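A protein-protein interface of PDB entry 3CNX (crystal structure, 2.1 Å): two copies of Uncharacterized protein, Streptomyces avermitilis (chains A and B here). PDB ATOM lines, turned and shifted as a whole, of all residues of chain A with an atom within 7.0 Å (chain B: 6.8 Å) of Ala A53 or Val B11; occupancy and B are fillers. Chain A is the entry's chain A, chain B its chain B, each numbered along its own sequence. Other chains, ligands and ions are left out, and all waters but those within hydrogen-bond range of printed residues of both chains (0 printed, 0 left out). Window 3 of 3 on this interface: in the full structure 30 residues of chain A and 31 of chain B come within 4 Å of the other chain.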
ATOM      1  N   PRO A  52     -15.142 -34.227 -10.945  1.00  0.00           N
ATOM      2  CA  PRO A  52     -14.072 -35.019 -10.341  1.00  0.00           C
ATOM      3  C   PRO A  52     -12.717 -34.355 -10.606  1.00  0.00           C
ATOM      4  O   PRO A  52     -11.772 -34.444  -9.813  1.00  0.00           O
ATOM      5  CB  PRO A  52     -14.207 -36.359 -11.065  1.00  0.00           C
ATOM      6  CG  PRO A  52     -15.727 -36.422 -11.503  1.00  0.00           C
ATOM      7  CD  PRO A  52     -16.315 -35.049 -11.296  1.00  0.00           C
ATOM      8  N   ALA A  53     -12.659 -33.683 -11.742  1.00  0.00           N
ATOM      9  CA  ALA A  53     -11.561 -32.789 -12.075  1.00  0.00           C
ATOM     10  C   ALA A  53     -12.239 -31.451 -12.074  1.00  0.00           C
ATOM     11  O   ALA A  53     -11.758 -30.476 -12.632  1.00  0.00           O
ATOM     12  CB  ALA A  53     -10.985 -33.100 -13.435  1.00  0.00           C
ATOM     13  N   ASP A  54     -13.398 -31.502 -11.427  1.00  0.00           N
ATOM     14  CA  ASP A  54     -14.371 -30.402 -11.253  1.00  0.00           C
ATOM     15  C   ASP A  54     -14.653 -29.619 -12.517  1.00  0.00           C
ATOM     16  O   ASP A  54     -14.759 -28.388 -12.497  1.00  0.00           O
ATOM     17  CB  ASP A  54     -13.969 -29.468 -10.118  1.00  0.00           C
ATOM     18  CG  ASP A  54     -14.453 -29.965  -8.775  1.00  0.00           C
ATOM     19  OD1 ASP A  54     -15.267 -30.910  -8.755  1.00  0.00           O
ATOM     20  OD2 ASP A  54     -14.026 -29.419  -7.738  1.00  0.00           O
ATOM     21  N   ALA A  55     -14.739 -30.369 -13.610  1.00  0.00           N
ATOM     22  CA  ALA A  55     -15.166 -29.852 -14.913  1.00  0.00           C
ATOM     23  C   ALA A  55     -16.429 -29.001 -14.820  1.00  0.00           C
ATOM     24  O   ALA A  55     -17.510 -29.494 -14.471  1.00  0.00           O
ATOM     25  CB  ALA A  55     -15.391 -31.002 -15.900  1.00  0.00           C
ATOM     26  N   GLY A  56     -16.277 -27.726 -15.161  1.00  0.00           N
ATOM     27  CA  GLY A  56     -17.404 -26.812 -15.310  1.00  0.00           C
ATOM     28  C   GLY A  56     -17.693 -26.016 -14.056  1.00  0.00           C
ATOM     29  O   GLY A  56     -18.504 -25.078 -14.078  1.00  0.00           O
ATOM     30  N   VAL A  57     -17.031 -26.403 -12.972  1.00  0.00           N
ATOM     31  CA  VAL A  57     -17.137 -25.696 -11.673  1.00  0.00           C
ATOM     32  C   VAL A  57     -16.626 -24.263 -11.727  1.00  0.00           C
ATOM     33  O   VAL A  57     -15.495 -23.984 -12.105  1.00  0.00           O
ATOM     34  CB  VAL A  57     -16.391 -26.402 -10.532  1.00  0.00           C
ATOM     35  CG1 VAL A  57     -16.318 -25.483  -9.318  1.00  0.00           C
ATOM     36  CG2 VAL A  57     -17.098 -27.695 -10.183  1.00  0.00           C
ATOM     37  N   TRP A 149     -17.359 -19.162 -16.717  1.00  0.00           N
ATOM     38  CA  TRP A 149     -16.705 -20.172 -15.913  1.00  0.00           C
ATOM     39  C   TRP A 149     -16.131 -19.465 -14.715  1.00  0.00           C
ATOM     40  O   TRP A 149     -16.157 -19.959 -13.589  1.00  0.00           O
ATOM     41  CB  TRP A 149     -15.635 -20.867 -16.745  1.00  0.00           C
ATOM     42  CG  TRP A 149     -14.936 -22.001 -16.119  1.00  0.00           C
ATOM     43  CD1 TRP A 149     -15.188 -22.560 -14.920  1.00  0.00           C
ATOM     44  CD2 TRP A 149     -13.871 -22.749 -16.706  1.00  0.00           C
ATOM     45  NE1 TRP A 149     -14.326 -23.607 -14.697  1.00  0.00           N
ATOM     46  CE2 TRP A 149     -13.523 -23.760 -15.799  1.00  0.00           C
ATOM     47  CE3 TRP A 149     -13.194 -22.675 -17.934  1.00  0.00           C
ATOM     48  CZ2 TRP A 149     -12.499 -24.684 -16.056  1.00  0.00           C
ATOM     49  CZ3 TRP A 149     -12.174 -23.581 -18.187  1.00  0.00           C
ATOM     50  CH2 TRP A 149     -11.825 -24.566 -17.244  1.00  0.00           C
ATOM     51  N   PRO B   7      -7.042 -36.871 -16.189  1.00  0.00           N
ATOM     52  CA  PRO B   7      -8.159 -36.605 -15.256  1.00  0.00           C
ATOM     53  C   PRO B   7      -7.673 -36.416 -13.824  1.00  0.00           C
ATOM     54  O   PRO B   7      -7.567 -35.283 -13.312  1.00  0.00           O
ATOM     55  CB  PRO B   7      -8.999 -37.885 -15.335  1.00  0.00           C
ATOM     56  CG  PRO B   7      -8.604 -38.522 -16.677  1.00  0.00           C
ATOM     57  CD  PRO B   7      -7.151 -38.184 -16.860  1.00  0.00           C
ATOM     58  N   ASP B   8      -7.393 -37.553 -13.194  1.00  0.00           N
ATOM     59  CA  ASP B   8      -6.757 -37.580 -11.879  1.00  0.00           C
ATOM     60  C   ASP B   8      -5.346 -37.077 -12.121  1.00  0.00           C
ATOM     61  O   ASP B   8      -4.698 -36.513 -11.240  1.00  0.00           O
ATOM     62  CB  ASP B   8      -6.743 -38.997 -11.292  1.00  0.00           C
ATOM     63  N   THR B   9      -4.908 -37.245 -13.362  1.00  0.00           N
ATOM     64  CA  THR B   9      -3.525 -36.931 -13.752  1.00  0.00           C
ATOM     65  C   THR B   9      -3.422 -35.487 -14.145  1.00  0.00           C
ATOM     66  O   THR B   9      -2.410 -34.820 -13.942  1.00  0.00           O
ATOM     67  CB  THR B   9      -3.057 -37.706 -14.981  1.00  0.00           C
ATOM     68  OG1 THR B   9      -2.692 -39.044 -14.608  1.00  0.00           O
ATOM     69  CG2 THR B   9      -1.859 -37.005 -15.599  1.00  0.00           C
ATOM     70  N   ASP B  10      -4.499 -35.043 -14.758  1.00  0.00           N
ATOM     71  CA  ASP B  10      -4.598 -33.665 -15.225  1.00  0.00           C
ATOM     72  C   ASP B  10      -4.535 -32.754 -14.037  1.00  0.00           C
ATOM     73  O   ASP B  10      -3.832 -31.755 -14.052  1.00  0.00           O
ATOM     74  CB  ASP B  10      -5.884 -33.417 -15.988  1.00  0.00           C
ATOM     75  CG  ASP B  10      -5.751 -33.733 -17.452  1.00  0.00           C
ATOM     76  OD1 ASP B  10      -4.612 -33.905 -17.927  1.00  0.00           O
ATOM     77  OD2 ASP B  10      -6.788 -33.794 -18.131  1.00  0.00           O
ATOM     78  N   VAL B  11      -5.259 -33.116 -12.993  1.00  0.00           N
ATOM     79  CA  VAL B  11      -5.325 -32.251 -11.827  1.00  0.00           C
ATOM     80  C   VAL B  11      -3.932 -32.125 -11.248  1.00  0.00           C
ATOM     81  O   VAL B  11      -3.512 -31.050 -10.858  1.00  0.00           O
ATOM     82  CB  VAL B  11      -6.297 -32.737 -10.758  1.00  0.00           C
ATOM     83  CG1 VAL B  11      -6.061 -31.968  -9.468  1.00  0.00           C
ATOM     84  CG2 VAL B  11      -7.708 -32.557 -11.229  1.00  0.00           C
ATOM     85  N   GLU B  12      -3.198 -33.231 -11.277  1.00  0.00           N
ATOM     86  CA  GLU B  12      -1.862 -33.317 -10.669  1.00  0.00           C
ATOM     87  C   GLU B  12      -0.849 -32.544 -11.514  1.00  0.00           C
ATOM     88  O   GLU B  12      -0.023 -31.786 -11.000  1.00  0.00           O
ATOM     89  CB  GLU B  12      -1.425 -34.775 -10.531  1.00  0.00           C
ATOM     90  N   GLN B  13      -0.944 -32.705 -12.824  1.00  0.00           N
ATOM     91  CA  GLN B  13      -0.035 -31.976 -13.716  1.00  0.00           C
ATOM     92  C   GLN B  13      -0.291 -30.477 -13.587  1.00  0.00           C
ATOM     93  O   GLN B  13       0.653 -29.703 -13.515  1.00  0.00           O
ATOM     94  CB  GLN B  13      -0.159 -32.416 -15.170  1.00  0.00           C
ATOM     95  CG  GLN B  13       0.192 -33.883 -15.437  1.00  0.00           C
ATOM     96  CD  GLN B  13       1.595 -34.270 -14.985  1.00  0.00           C
ATOM     97  OE1 GLN B  13       2.502 -33.442 -14.923  1.00  0.00           O
ATOM     98  NE2 GLN B  13       1.775 -35.555 -14.672  1.00  0.00           N
ATOM     99  N   VAL B  14      -1.561 -30.070 -13.525  1.00  0.00           N
ATOM    100  CA  VAL B  14      -1.897 -28.624 -13.452  1.00  0.00           C
ATOM    101  C   VAL B  14      -1.348 -28.063 -12.144  1.00  0.00           C
ATOM    102  O   VAL B  14      -0.811 -26.953 -12.059  1.00  0.00           O
ATOM    103  CB  VAL B  14      -3.427 -28.332 -13.656  1.00  0.00           C
ATOM    104  CG1 VAL B  14      -3.824 -26.926 -13.166  1.00  0.00           C
ATOM    105  CG2 VAL B  14      -3.776 -28.439 -15.122  1.00  0.00           C
ATOM    106  N   GLY B  15      -1.421 -28.894 -11.127  1.00  0.00           N
ATOM    107  CA  GLY B  15      -1.030 -28.499  -9.777  1.00  0.00           C
ATOM    108  C   GLY B  15       0.444 -28.246  -9.782  1.00  0.00           C
ATOM    109  O   GLY B  15       0.958 -27.308  -9.140  1.00  0.00           O
ATOM    110  N   LEU B  16       1.111 -29.067 -10.578  1.00  0.00           N
ATOM    111  CA  LEU B  16       2.572 -29.060 -10.660  1.00  0.00           C
ATOM    112  C   LEU B  16       3.004 -27.777 -11.379  1.00  0.00           C
ATOM    113  O   LEU B  16       3.953 -27.091 -10.978  1.00  0.00           O
ATOM    114  CB  LEU B  16       3.101 -30.328 -11.363  1.00  0.00           C
ATOM    115  CG  LEU B  16       3.114 -31.587 -10.473  1.00  0.00           C
ATOM    116  CD1 LEU B  16       3.480 -32.884 -11.230  1.00  0.00           C
ATOM    117  CD2 LEU B  16       4.057 -31.391  -9.290  1.00  0.00           C
ATOM    118  N   HIS B  96      -7.655 -24.838  -5.557  1.00  0.00           N
ATOM    119  CA  HIS B  96      -8.652 -25.647  -6.261  1.00  0.00           C
ATOM    120  C   HIS B  96      -8.461 -25.665  -7.762  1.00  0.00           C
ATOM    121  O   HIS B  96      -8.308 -24.646  -8.398  1.00  0.00           O
ATOM    122  CB  HIS B  96     -10.071 -25.214  -5.871  1.00  0.00           C
ATOM    123  CG  HIS B  96     -11.139 -25.858  -6.694  1.00  0.00           C
ATOM    124  ND1 HIS B  96     -11.572 -25.321  -7.889  1.00  0.00           N
ATOM    125  CD2 HIS B  96     -11.845 -27.003  -6.515  1.00  0.00           C
ATOM    126  CE1 HIS B  96     -12.510 -26.103  -8.404  1.00  0.00           C
ATOM    127  NE2 HIS B  96     -12.690 -27.130  -7.592  1.00  0.00           N
ATOM    128  N   VAL B  97      -8.514 -26.869  -8.315  1.00  0.00           N
ATOM    129  CA  VAL B  97      -8.344 -27.091  -9.769  1.00  0.00           C
ATOM    130  C   VAL B  97      -9.583 -27.622 -10.487  1.00  0.00           C
ATOM    131  O   VAL B  97     -10.233 -28.579 -10.075  1.00  0.00           O
ATOM    132  CB  VAL B  97      -7.159 -28.063 -10.055  1.00  0.00           C
ATOM    133  CG1 VAL B  97      -7.000 -28.280 -11.556  1.00  0.00           C
ATOM    134  CG2 VAL B  97      -5.865 -27.539  -9.425  1.00  0.00           C
ATOM    135  N   SER B  98      -9.889 -26.977 -11.597  1.00  0.00           N
ATOM    136  CA  SER B  98     -10.982 -27.385 -12.456  1.00  0.00           C
ATOM    137  C   SER B  98     -10.491 -27.527 -13.890  1.00  0.00           C
ATOM    138  O   SER B  98     -10.079 -26.570 -14.505  1.00  0.00           O
ATOM    139  CB  SER B  98     -12.127 -26.364 -12.365  1.00  0.00           C
ATOM    140  OG  SER B  98     -13.054 -26.488 -13.434  1.00  0.00           O
ATOM    141  N   VAL B  99     -10.525 -28.747 -14.400  1.00  0.00           N
ATOM    142  CA  VAL B  99     -10.060 -29.028 -15.757  1.00  0.00           C
ATOM    143  C   VAL B  99     -11.248 -29.301 -16.647  1.00  0.00           C
ATOM    144  O   VAL B  99     -12.135 -30.080 -16.305  1.00  0.00           O
ATOM    145  CB  VAL B  99      -9.061 -30.200 -15.775  1.00  0.00           C
ATOM    146  CG1 VAL B  99      -8.357 -30.263 -17.109  1.00  0.00           C
ATOM    147  CG2 VAL B  99      -8.033 -30.038 -14.647  1.00  0.00           C
ATOM    148  N   THR B 100     -11.277 -28.583 -17.763  1.00  0.00           N
ATOM    149  CA  THR B 100     -12.285 -28.758 -18.795  1.00  0.00           C
ATOM    150  C   THR B 100     -11.648 -28.775 -20.172  1.00  0.00           C
ATOM    151  O   THR B 100     -11.288 -27.745 -20.707  1.00  0.00           O
ATOM    152  CB  THR B 100     -13.329 -27.615 -18.765  1.00  0.00           C
ATOM    153  OG1 THR B 100     -13.808 -27.434 -17.422  1.00  0.00           O
ATOM    154  CG2 THR B 100     -14.499 -27.919 -19.687  1.00  0.00           C
ATOM    155  N   LEU B 105      -8.587 -24.240 -14.740  1.00  0.00           N
ATOM    156  CA  LEU B 105      -8.790 -23.078 -13.885  1.00  0.00           C
ATOM    157  C   LEU B 105      -8.415 -23.441 -12.472  1.00  0.00           C
ATOM    158  O   LEU B 105      -8.923 -24.396 -11.889  1.00  0.00           O
ATOM    159  CB  LEU B 105     -10.241 -22.662 -13.915  1.00  0.00           C
ATOM    160  CG  LEU B 105     -10.620 -21.235 -13.588  1.00  0.00           C
ATOM    161  CD1 LEU B 105     -10.382 -20.419 -14.801  1.00  0.00           C
ATOM    162  CD2 LEU B 105     -12.108 -21.255 -13.216  1.00  0.00           C
ATOM    163  N   TRP B 146       1.399 -27.773 -19.339  1.00  0.00           N
ATOM    164  CA  TRP B 146       0.416 -26.771 -18.995  1.00  0.00           C
ATOM    165  C   TRP B 146       1.144 -25.462 -18.872  1.00  0.00           C
ATOM    166  O   TRP B 146       2.153 -25.349 -18.185  1.00  0.00           O
ATOM    167  CB  TRP B 146      -0.349 -27.119 -17.704  1.00  0.00           C
ATOM    168  CG  TRP B 146      -1.252 -28.345 -17.859  1.00  0.00           C
ATOM    169  CD1 TRP B 146      -0.911 -29.642 -17.625  1.00  0.00           C
ATOM    170  CD2 TRP B 146      -2.615 -28.366 -18.291  1.00  0.00           C
ATOM    171  NE1 TRP B 146      -1.974 -30.468 -17.876  1.00  0.00           N
ATOM    172  CE2 TRP B 146      -3.032 -29.707 -18.297  1.00  0.00           C
ATOM    173  CE3 TRP B 146      -3.519 -27.382 -18.691  1.00  0.00           C
ATOM    174  CZ2 TRP B 146      -4.310 -30.089 -18.672  1.00  0.00           C
ATOM    175  CZ3 TRP B 146      -4.804 -27.775 -19.062  1.00  0.00           C
ATOM    176  CH2 TRP B 146      -5.182 -29.105 -19.042  1.00  0.00           C
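Among the printed residues, pairs that only touch across the chains: Ala A53 with Ser B98 (3.2 Å), Trp A149 with Thr B100 (3.3 Å), Ala A55 with Val B99 (3.3 Å), Ala A53 with Val B97 (3.5 Å), Trp A149 with Leu B105 (3.6 Å), Ala A55 with Thr B100 (3.7 Å), Val A57 with Ser B98 (3.7 Å), Asp A54 with Val B97 (3.8 Å), Gly A56 with Ser B98 (3.9 Å), Ala A53 with Val B11 (3.95 Å) and Val A57 with His B96 (3.96 Å).
OD2 of Asp A54 is in hydrogen-bond range of NE2 of His B96, at 2.7 Å. O of Asp A54 is in hydrogen-bond range of OG of Ser B98, 2.7 Å away. NE1 of Trp A149 lies close to OG of Ser B98. The backbone NH (N) of Gly A56 is in hydrogen-bond range of the side-chain hydroxyl (OG1) of Thr B100, 3.4 Å away. The backbone carbonyl oxygen (O) of Ala A53 lies within hydrogen-bond range of the backbone NH (N) of Val B99 (2.8 Å).
The backbone NH (N) of Ser B98 is in hydrogen-bond range of the backbone carbonyl oxygen (O) of Leu B105 (2.8 Å). O of Val A57 is in hydrogen-bond range of NE1 of Trp A149.
Of the 7 printed residues of chain A, 6 touch a printed residue of chain B. Printed residues of chain A that touch a printed residue of chain B: Ala A53, Asp A54, Ala A55, Gly A56, Val A57 and Trp A149. Hydrophobic or aromatic side chains of chain A within 4 Å of the printed part of chain B: Ala A53, Ala A55, Val A57 and Trp A149. Of the 17 printed residues of chain B, 7 touch a printed residue of chain A. Hydrophobic or aromatic side chains of chain B within 4 Å of the printed part of chain A: Val B11, His B96 and Leu B105. Among the printed residues, 16 pairs touch across the chains. Among the printed residues, no Asp or Glu carboxylate lies within 4 Å of a Lys or Arg side-chain nitrogen of the other chain.
No position is printed for both chains. Of the 16 pairs that touch across the chains among the printed residues, none has its exchanged pair printed and touching as well.
Ala A53 touches four residues of chain B. Val B11 touches just one residue of chain A: Ala A53 (3.95 Å). Printed residues of chain A within 4 Å of Val B99: Ala A53 and Ala A55. Of the printed residues of chain A, Thr B100 touches Ala A55, Gly A56 and Trp A149. Of the printed residues of chain A, His B96 touches Asp A54 and Val A57. Thr B9 touches none of the printed residues of chain A. Gly B15 touches none of the printed residues of chain A.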
